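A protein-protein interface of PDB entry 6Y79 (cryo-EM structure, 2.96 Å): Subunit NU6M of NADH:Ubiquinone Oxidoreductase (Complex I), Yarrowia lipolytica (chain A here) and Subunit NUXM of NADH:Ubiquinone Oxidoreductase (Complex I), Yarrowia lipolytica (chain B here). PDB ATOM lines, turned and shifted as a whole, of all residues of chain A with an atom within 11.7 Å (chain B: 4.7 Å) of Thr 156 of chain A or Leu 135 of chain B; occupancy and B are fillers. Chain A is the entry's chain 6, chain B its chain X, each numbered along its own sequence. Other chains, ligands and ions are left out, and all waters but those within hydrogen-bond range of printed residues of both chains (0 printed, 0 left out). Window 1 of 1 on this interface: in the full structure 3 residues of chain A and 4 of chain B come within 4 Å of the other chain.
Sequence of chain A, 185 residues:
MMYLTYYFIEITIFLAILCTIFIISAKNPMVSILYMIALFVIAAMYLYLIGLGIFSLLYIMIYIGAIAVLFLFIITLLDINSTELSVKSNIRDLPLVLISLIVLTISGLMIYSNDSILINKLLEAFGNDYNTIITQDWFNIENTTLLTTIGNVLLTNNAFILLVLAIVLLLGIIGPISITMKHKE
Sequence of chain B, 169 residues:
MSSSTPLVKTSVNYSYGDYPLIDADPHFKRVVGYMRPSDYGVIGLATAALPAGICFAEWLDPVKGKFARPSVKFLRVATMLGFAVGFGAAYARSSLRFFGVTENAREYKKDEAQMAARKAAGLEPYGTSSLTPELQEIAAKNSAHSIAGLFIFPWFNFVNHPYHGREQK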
ATOM      1  N   GLU A 142      23.104 -15.692  -8.613  1.00  0.00           N
ATOM      2  CA  GLU A 142      22.920 -16.324  -7.315  1.00  0.00           C
ATOM      3  C   GLU A 142      23.189 -17.819  -7.371  1.00  0.00           C
ATOM      4  O   GLU A 142      23.273 -18.422  -8.442  1.00  0.00           O
ATOM      5  CB  GLU A 142      21.521 -16.079  -6.777  1.00  0.00           C
ATOM      6  CG  GLU A 142      20.435 -16.400  -7.747  1.00  0.00           C
ATOM      7  CD  GLU A 142      19.084 -16.196  -7.126  1.00  0.00           C
ATOM      8  OE1 GLU A 142      19.022 -15.559  -6.054  1.00  0.00           O
ATOM      9  OE2 GLU A 142      18.086 -16.679  -7.694  1.00  0.00           O
ATOM     10  N   THR A 144      21.858 -20.639  -7.295  1.00  0.00           N
ATOM     11  CA  THR A 144      20.892 -21.657  -7.661  1.00  0.00           C
ATOM     12  C   THR A 144      21.672 -22.826  -8.227  1.00  0.00           C
ATOM     13  O   THR A 144      22.055 -22.831  -9.397  1.00  0.00           O
ATOM     14  CB  THR A 144      19.882 -21.121  -8.662  1.00  0.00           C
ATOM     15  OG1 THR A 144      19.281 -19.932  -8.142  1.00  0.00           O
ATOM     16  CG2 THR A 144      18.804 -22.148  -8.865  1.00  0.00           C
ATOM     17  N   LEU A 147      20.027 -28.801  -7.025  1.00  0.00           N
ATOM     18  CA  LEU A 147      19.033 -29.234  -6.051  1.00  0.00           C
ATOM     19  C   LEU A 147      17.996 -28.148  -5.790  1.00  0.00           C
ATOM     20  O   LEU A 147      16.828 -28.455  -5.526  1.00  0.00           O
ATOM     21  CB  LEU A 147      19.738 -29.642  -4.761  1.00  0.00           C
ATOM     22  CG  LEU A 147      18.927 -30.381  -3.705  1.00  0.00           C
ATOM     23  CD1 LEU A 147      18.387 -31.671  -4.267  1.00  0.00           C
ATOM     24  CD2 LEU A 147      19.794 -30.652  -2.502  1.00  0.00           C
ATOM     25  N   THR A 148      18.395 -26.882  -5.915  1.00  0.00           N
ATOM     26  CA  THR A 148      17.454 -25.777  -5.795  1.00  0.00           C
ATOM     27  C   THR A 148      16.444 -25.772  -6.934  1.00  0.00           C
ATOM     28  O   THR A 148      15.248 -25.560  -6.710  1.00  0.00           O
ATOM     29  CB  THR A 148      18.218 -24.457  -5.754  1.00  0.00           C
ATOM     30  OG1 THR A 148      19.117 -24.466  -4.641  1.00  0.00           O
ATOM     31  CG2 THR A 148      17.262 -23.293  -5.609  1.00  0.00           C
ATOM     32  N   THR A 149      16.892 -26.030  -8.164  1.00  0.00           N
ATOM     33  CA  THR A 149      15.953 -25.998  -9.275  1.00  0.00           C
ATOM     34  C   THR A 149      15.078 -27.244  -9.291  1.00  0.00           C
ATOM     35  O   THR A 149      13.912 -27.168  -9.700  1.00  0.00           O
ATOM     36  CB  THR A 149      16.701 -25.833 -10.592  1.00  0.00           C
ATOM     37  OG1 THR A 149      17.702 -24.830 -10.426  1.00  0.00           O
ATOM     38  CG2 THR A 149      15.730 -25.391 -11.687  1.00  0.00           C
ATOM     39  N   ILE A 150      15.599 -28.383  -8.817  1.00  0.00           N
ATOM     40  CA  ILE A 150      14.744 -29.553  -8.619  1.00  0.00           C
ATOM     41  C   ILE A 150      13.672 -29.254  -7.578  1.00  0.00           C
ATOM     42  O   ILE A 150      12.498 -29.598  -7.755  1.00  0.00           O
ATOM     43  CB  ILE A 150      15.581 -30.791  -8.241  1.00  0.00           C
ATOM     44  CG1 ILE A 150      16.416 -31.245  -9.430  1.00  0.00           C
ATOM     45  CG2 ILE A 150      14.694 -31.946  -7.844  1.00  0.00           C
ATOM     46  CD1 ILE A 150      17.282 -32.440  -9.137  1.00  0.00           C
ATOM     47  N   GLY A 151      14.037 -28.546  -6.515  1.00  0.00           N
ATOM     48  CA  GLY A 151      13.033 -28.117  -5.565  1.00  0.00           C
ATOM     49  C   GLY A 151      12.111 -27.017  -6.049  1.00  0.00           C
ATOM     50  O   GLY A 151      11.060 -26.820  -5.438  1.00  0.00           O
ATOM     51  N   ASN A 152      12.479 -26.267  -7.081  1.00  0.00           N
ATOM     52  CA  ASN A 152      11.530 -25.298  -7.614  1.00  0.00           C
ATOM     53  C   ASN A 152      10.527 -25.960  -8.531  1.00  0.00           C
ATOM     54  O   ASN A 152       9.347 -25.615  -8.502  1.00  0.00           O
ATOM     55  CB  ASN A 152      12.257 -24.184  -8.380  1.00  0.00           C
ATOM     56  CG  ASN A 152      11.375 -22.969  -8.687  1.00  0.00           C
ATOM     57  OD1 ASN A 152      10.212 -22.895  -8.287  1.00  0.00           O
ATOM     58  ND2 ASN A 152      11.922 -22.024  -9.448  1.00  0.00           N
ATOM     59  N   VAL A 153      10.952 -26.954  -9.299  1.00  0.00           N
ATOM     60  CA  VAL A 153      10.073 -27.481 -10.329  1.00  0.00           C
ATOM     61  C   VAL A 153       9.312 -28.729  -9.873  1.00  0.00           C
ATOM     62  O   VAL A 153       8.208 -28.982 -10.356  1.00  0.00           O
ATOM     63  CB  VAL A 153      10.913 -27.696 -11.592  1.00  0.00           C
ATOM     64  CG1 VAL A 153      10.056 -28.024 -12.751  1.00  0.00           C
ATOM     65  CG2 VAL A 153      11.575 -26.395 -11.899  1.00  0.00           C
ATOM     66  N   LEU A 154       9.811 -29.464  -8.875  1.00  0.00           N
ATOM     67  CA  LEU A 154       8.953 -30.415  -8.172  1.00  0.00           C
ATOM     68  C   LEU A 154       7.821 -29.735  -7.420  1.00  0.00           C
ATOM     69  O   LEU A 154       6.826 -30.388  -7.105  1.00  0.00           O
ATOM     70  CB  LEU A 154       9.740 -31.233  -7.156  1.00  0.00           C
ATOM     71  CG  LEU A 154      10.565 -32.448  -7.534  1.00  0.00           C
ATOM     72  CD1 LEU A 154      11.335 -32.888  -6.306  1.00  0.00           C
ATOM     73  CD2 LEU A 154       9.661 -33.549  -8.025  1.00  0.00           C
ATOM     74  N   LEU A 155       7.955 -28.449  -7.110  1.00  0.00           N
ATOM     75  CA  LEU A 155       7.065 -27.789  -6.174  1.00  0.00           C
ATOM     76  C   LEU A 155       6.154 -26.751  -6.799  1.00  0.00           C
ATOM     77  O   LEU A 155       5.192 -26.336  -6.150  1.00  0.00           O
ATOM     78  CB  LEU A 155       7.871 -27.110  -5.062  1.00  0.00           C
ATOM     79  CG  LEU A 155       8.251 -27.939  -3.836  1.00  0.00           C
ATOM     80  CD1 LEU A 155       6.967 -28.461  -3.326  1.00  0.00           C
ATOM     81  CD2 LEU A 155       9.225 -29.084  -4.054  1.00  0.00           C
ATOM     82  N   THR A 156       6.448 -26.296  -8.010  1.00  0.00           N
ATOM     83  CA  THR A 156       5.586 -25.349  -8.702  1.00  0.00           C
ATOM     84  C   THR A 156       5.011 -25.925  -9.984  1.00  0.00           C
ATOM     85  O   THR A 156       3.790 -26.000 -10.129  1.00  0.00           O
ATOM     86  CB  THR A 156       6.372 -24.077  -9.007  1.00  0.00           C
ATOM     87  OG1 THR A 156       7.671 -24.422  -9.499  1.00  0.00           O
ATOM     88  CG2 THR A 156       6.496 -23.250  -7.783  1.00  0.00           C
ATOM     89  N   ASN A 157       5.863 -26.350 -10.907  1.00  0.00           N
ATOM     90  CA  ASN A 157       5.403 -26.774 -12.216  1.00  0.00           C
ATOM     91  C   ASN A 157       4.956 -28.221 -12.214  1.00  0.00           C
ATOM     92  O   ASN A 157       4.073 -28.596 -12.991  1.00  0.00           O
ATOM     93  CB  ASN A 157       6.519 -26.575 -13.229  1.00  0.00           C
ATOM     94  CG  ASN A 157       6.846 -25.132 -13.444  1.00  0.00           C
ATOM     95  OD1 ASN A 157       5.991 -24.347 -13.835  1.00  0.00           O
ATOM     96  ND2 ASN A 157       8.085 -24.762 -13.183  1.00  0.00           N
ATOM     97  N   ASN A 158       5.546 -29.038 -11.356  1.00  0.00           N
ATOM     98  CA  ASN A 158       5.228 -30.448 -11.266  1.00  0.00           C
ATOM     99  C   ASN A 158       4.852 -30.800  -9.846  1.00  0.00           C
ATOM    100  O   ASN A 158       5.312 -31.795  -9.287  1.00  0.00           O
ATOM    101  CB  ASN A 158       6.394 -31.287 -11.768  1.00  0.00           C
ATOM    102  CG  ASN A 158       6.750 -30.959 -13.188  1.00  0.00           C
ATOM    103  OD1 ASN A 158       7.771 -30.352 -13.452  1.00  0.00           O
ATOM    104  ND2 ASN A 158       5.896 -31.346 -14.112  1.00  0.00           N
ATOM    105  N   ALA A 159       4.012 -29.959  -9.243  1.00  0.00           N
ATOM    106  CA  ALA A 159       3.533 -30.200  -7.888  1.00  0.00           C
ATOM    107  C   ALA A 159       2.605 -31.401  -7.842  1.00  0.00           C
ATOM    108  O   ALA A 159       2.596 -32.161  -6.864  1.00  0.00           O
ATOM    109  CB  ALA A 159       2.822 -28.954  -7.373  1.00  0.00           C
ATOM    110  N   PHE A 160       1.822 -31.590  -8.904  1.00  0.00           N
ATOM    111  CA  PHE A 160       0.931 -32.734  -9.001  1.00  0.00           C
ATOM    112  C   PHE A 160       1.706 -34.040  -9.081  1.00  0.00           C
ATOM    113  O   PHE A 160       1.249 -35.055  -8.547  1.00  0.00           O
ATOM    114  CB  PHE A 160       0.023 -32.556 -10.215  1.00  0.00           C
ATOM    115  CG  PHE A 160      -0.959 -33.662 -10.410  1.00  0.00           C
ATOM    116  CD1 PHE A 160      -2.117 -33.712  -9.660  1.00  0.00           C
ATOM    117  CD2 PHE A 160      -0.731 -34.644 -11.354  1.00  0.00           C
ATOM    118  CE1 PHE A 160      -3.016 -34.723  -9.839  1.00  0.00           C
ATOM    119  CE2 PHE A 160      -1.626 -35.657 -11.530  1.00  0.00           C
ATOM    120  CZ  PHE A 160      -2.771 -35.695 -10.773  1.00  0.00           C
ATOM    121  N   ILE A 161       2.880 -34.030  -9.719  1.00  0.00           N
ATOM    122  CA  ILE A 161       3.720 -35.223  -9.772  1.00  0.00           C
ATOM    123  C   ILE A 161       4.245 -35.562  -8.388  1.00  0.00           C
ATOM    124  O   ILE A 161       4.294 -36.731  -8.000  1.00  0.00           O
ATOM    125  CB  ILE A 161       4.859 -35.021 -10.784  1.00  0.00           C
ATOM    126  CG1 ILE A 161       4.283 -34.911 -12.184  1.00  0.00           C
ATOM    127  CG2 ILE A 161       5.852 -36.165 -10.759  1.00  0.00           C
ATOM    128  CD1 ILE A 161       5.293 -34.569 -13.194  1.00  0.00           C
ATOM    129  N   LEU A 162       4.568 -34.539  -7.598  1.00  0.00           N
ATOM    130  CA  LEU A 162       4.991 -34.744  -6.218  1.00  0.00           C
ATOM    131  C   LEU A 162       3.865 -35.294  -5.352  1.00  0.00           C
ATOM    132  O   LEU A 162       4.107 -36.150  -4.496  1.00  0.00           O
ATOM    133  CB  LEU A 162       5.542 -33.427  -5.672  1.00  0.00           C
ATOM    134  CG  LEU A 162       6.185 -33.262  -4.300  1.00  0.00           C
ATOM    135  CD1 LEU A 162       7.382 -32.370  -4.445  1.00  0.00           C
ATOM    136  CD2 LEU A 162       5.203 -32.607  -3.351  1.00  0.00           C
ATOM    137  N   LEU A 163       2.621 -34.890  -5.604  1.00  0.00           N
ATOM    138  CA  LEU A 163       1.529 -35.403  -4.778  1.00  0.00           C
ATOM    139  C   LEU A 163       1.087 -36.813  -5.191  1.00  0.00           C
ATOM    140  O   LEU A 163       0.742 -37.644  -4.337  1.00  0.00           O
ATOM    141  CB  LEU A 163       0.362 -34.424  -4.811  1.00  0.00           C
ATOM    142  CG  LEU A 163       0.620 -33.018  -4.253  1.00  0.00           C
ATOM    143  CD1 LEU A 163      -0.677 -32.354  -3.924  1.00  0.00           C
ATOM    144  CD2 LEU A 163       1.486 -33.042  -3.018  1.00  0.00           C
ATOM    145  N   LEU B 131       2.581 -13.136  -3.683  1.00  0.00           N
ATOM    146  CA  LEU B 131       3.412 -13.942  -4.559  1.00  0.00           C
ATOM    147  C   LEU B 131       4.062 -13.039  -5.592  1.00  0.00           C
ATOM    148  O   LEU B 131       3.533 -11.980  -5.938  1.00  0.00           O
ATOM    149  CB  LEU B 131       2.614 -15.035  -5.280  1.00  0.00           C
ATOM    150  CG  LEU B 131       1.973 -16.213  -4.549  1.00  0.00           C
ATOM    151  CD1 LEU B 131       1.241 -17.078  -5.526  1.00  0.00           C
ATOM    152  CD2 LEU B 131       3.003 -17.039  -3.859  1.00  0.00           C
ATOM    153  N   THR B 132       5.222 -13.465  -6.072  1.00  0.00           N
ATOM    154  CA  THR B 132       5.818 -12.825  -7.225  1.00  0.00           C
ATOM    155  C   THR B 132       4.989 -13.175  -8.458  1.00  0.00           C
ATOM    156  O   THR B 132       4.296 -14.194  -8.459  1.00  0.00           O
ATOM    157  CB  THR B 132       7.264 -13.283  -7.378  1.00  0.00           C
ATOM    158  OG1 THR B 132       7.300 -14.687  -7.645  1.00  0.00           O
ATOM    159  CG2 THR B 132       8.026 -13.005  -6.101  1.00  0.00           C
ATOM    160  N   PRO B 133       4.995 -12.328  -9.500  1.00  0.00           N
ATOM    161  CA  PRO B 133       4.136 -12.609 -10.667  1.00  0.00           C
ATOM    162  C   PRO B 133       4.491 -13.882 -11.419  1.00  0.00           C
ATOM    163  O   PRO B 133       3.609 -14.474 -12.057  1.00  0.00           O
ATOM    164  CB  PRO B 133       4.329 -11.361 -11.538  1.00  0.00           C
ATOM    165  CG  PRO B 133       5.619 -10.798 -11.101  1.00  0.00           C
ATOM    166  CD  PRO B 133       5.616 -11.001  -9.632  1.00  0.00           C
ATOM    167  N   GLU B 134       5.746 -14.333 -11.330  1.00  0.00           N
ATOM    168  CA  GLU B 134       6.128 -15.652 -11.822  1.00  0.00           C
ATOM    169  C   GLU B 134       5.380 -16.759 -11.090  1.00  0.00           C
ATOM    170  O   GLU B 134       4.845 -17.682 -11.717  1.00  0.00           O
ATOM    171  CB  GLU B 134       7.632 -15.845 -11.651  1.00  0.00           C
ATOM    172  CG  GLU B 134       8.486 -15.202 -12.724  1.00  0.00           C
ATOM    173  CD  GLU B 134       8.967 -13.812 -12.341  1.00  0.00           C
ATOM    174  OE1 GLU B 134       8.556 -13.299 -11.279  1.00  0.00           O
ATOM    175  OE2 GLU B 134       9.762 -13.231 -13.109  1.00  0.00           O
ATOM    176  N   LEU B 135       5.334 -16.677  -9.760  1.00  0.00           N
ATOM    177  CA  LEU B 135       4.637 -17.686  -8.975  1.00  0.00           C
ATOM    178  C   LEU B 135       3.132 -17.591  -9.136  1.00  0.00           C
ATOM    179  O   LEU B 135       2.457 -18.619  -9.086  1.00  0.00           O
ATOM    180  CB  LEU B 135       4.997 -17.563  -7.504  1.00  0.00           C
ATOM    181  CG  LEU B 135       6.390 -18.016  -7.116  1.00  0.00           C
ATOM    182  CD1 LEU B 135       6.632 -17.693  -5.662  1.00  0.00           C
ATOM    183  CD2 LEU B 135       6.522 -19.490  -7.372  1.00  0.00           C
ATOM    184  N   GLN B 136       2.592 -16.383  -9.321  1.00  0.00           N
ATOM    185  CA  GLN B 136       1.172 -16.237  -9.629  1.00  0.00           C
ATOM    186  C   GLN B 136       0.835 -16.905 -10.951  1.00  0.00           C
ATOM    187  O   GLN B 136      -0.188 -17.590 -11.071  1.00  0.00           O
ATOM    188  CB  GLN B 136       0.785 -14.764  -9.688  1.00  0.00           C
ATOM    189  CG  GLN B 136       0.816 -14.030  -8.389  1.00  0.00           C
ATOM    190  CD  GLN B 136       0.638 -12.553  -8.596  1.00  0.00           C
ATOM    191  OE1 GLN B 136       0.392 -12.102  -9.709  1.00  0.00           O
ATOM    192  NE2 GLN B 136       0.786 -11.784  -7.535  1.00  0.00           N
ATOM    193  N   GLU B 137       1.713 -16.745 -11.943  1.00  0.00           N
ATOM    194  CA  GLU B 137       1.467 -17.337 -13.250  1.00  0.00           C
ATOM    195  C   GLU B 137       1.533 -18.857 -13.203  1.00  0.00           C
ATOM    196  O   GLU B 137       0.673 -19.537 -13.773  1.00  0.00           O
ATOM    197  CB  GLU B 137       2.451 -16.799 -14.278  1.00  0.00           C
ATOM    198  CG  GLU B 137       2.199 -17.343 -15.661  1.00  0.00           C
ATOM    199  CD  GLU B 137       3.325 -17.051 -16.617  1.00  0.00           C
ATOM    200  OE1 GLU B 137       4.132 -16.144 -16.329  1.00  0.00           O
ATOM    201  OE2 GLU B 137       3.415 -17.740 -17.652  1.00  0.00           O
ATOM    202  N   ILE B 138       2.534 -19.406 -12.514  1.00  0.00           N
ATOM    203  CA  ILE B 138       2.649 -20.859 -12.400  1.00  0.00           C
ATOM    204  C   ILE B 138       1.505 -21.427 -11.561  1.00  0.00           C
ATOM    205  O   ILE B 138       0.935 -22.480 -11.885  1.00  0.00           O
ATOM    206  CB  ILE B 138       4.028 -21.219 -11.821  1.00  0.00           C
ATOM    207  CG1 ILE B 138       5.131 -20.794 -12.780  1.00  0.00           C
ATOM    208  CG2 ILE B 138       4.149 -22.685 -11.590  1.00  0.00           C
ATOM    209  CD1 ILE B 138       6.501 -20.838 -12.165  1.00  0.00           C
ATOM    210  N   ALA B 139       1.110 -20.703 -10.513  1.00  0.00           N
ATOM    211  CA  ALA B 139       0.051 -21.148  -9.621  1.00  0.00           C
ATOM    212  C   ALA B 139      -1.301 -21.152 -10.308  1.00  0.00           C
ATOM    213  O   ALA B 139      -2.183 -21.940  -9.950  1.00  0.00           O
ATOM    214  CB  ALA B 139       0.011 -20.238  -8.403  1.00  0.00           C
ATOM    215  N   ASN B 142      -1.459 -24.078 -12.749  1.00  0.00           N
ATOM    216  CA  ASN B 142      -1.796 -25.320 -12.062  1.00  0.00           C
ATOM    217  C   ASN B 142      -3.303 -25.475 -11.893  1.00  0.00           C
ATOM    218  O   ASN B 142      -3.852 -26.548 -12.149  1.00  0.00           O
ATOM    219  CB  ASN B 142      -1.101 -25.385 -10.705  1.00  0.00           C
ATOM    220  CG  ASN B 142       0.347 -25.785 -10.810  1.00  0.00           C
ATOM    221  OD1 ASN B 142       0.725 -26.569 -11.670  1.00  0.00           O
ATOM    222  ND2 ASN B 142       1.166 -25.263  -9.919  1.00  0.00           N
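The side-chain amide nitrogen (ND2) of Asn 142 of chain B lies within hydrogen-bond range of the backbone carbonyl oxygen (O) of Thr 156 of chain A (2.7 Å).
The backbone carbonyl oxygen (O) of Ile 138 of chain B is in hydrogen-bond range of the side-chain amide nitrogen (ND2) of Asn 142 of chain B.
OG1 of Thr 156 of chain A lies within hydrogen-bond range of OD1 of Asn 152 of chain A (3.2 Å).
CG2 of Thr 156 of chain A touches CD2 of Leu 135 of chain B, 3.8 Å away.
Ile 138 of chain B touches Thr 156 of chain A.
OD1 of Asn 157 of chain A touches CG2 of Ile 138 of chain B (3.3 Å).
Of the printed residues of chain B, Thr 156 of chain A touches Leu 135 (3.8 Å), Ile 138 (3.6 Å) and Asn 142 (2.7 Å).
Printed residues of chain B within 4 Å of Asn 157 of chain A: Ile 138.
No residue of chain A comes within 4 Å of Leu 131 of chain B.
No residue of chain A comes within 4 Å of Thr 132 of chain B.
No residue of chain A comes within 4 Å of Pro 133 of chain B.
No residue of chain A comes within 4 Å of Glu 134 of chain B.
Leu 135 of chain B touches just one residue of chain A: Thr 156.
No residue of chain A comes within 4 Å of Gln 136 of chain B.
Of chain A, only Thr 156 and Asn 157 come within 4 Å of Ile 138 of chain B.
No residue of chain A comes within 4 Å of Ala 139 of chain B.
Printed residues of chain A within 4 Å of Asn 142 of chain B: Thr 156.
The nearest printed residue of chain B that does not touch Asn 157 of chain A is Asn 142 of chain B (4.1 Å).
Of the 10 printed residues of chain B, 3 touch a printed residue of chain A.
Printed residues of chain B that touch a printed residue of chain A: Leu 135, Ile 138 and Asn 142.
Among the printed residues, 4 pairs touch across the chains.
Among the printed residues, no Asp or Glu carboxylate lies within 4 Å of a Lys or Arg side-chain nitrogen of the other chain.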
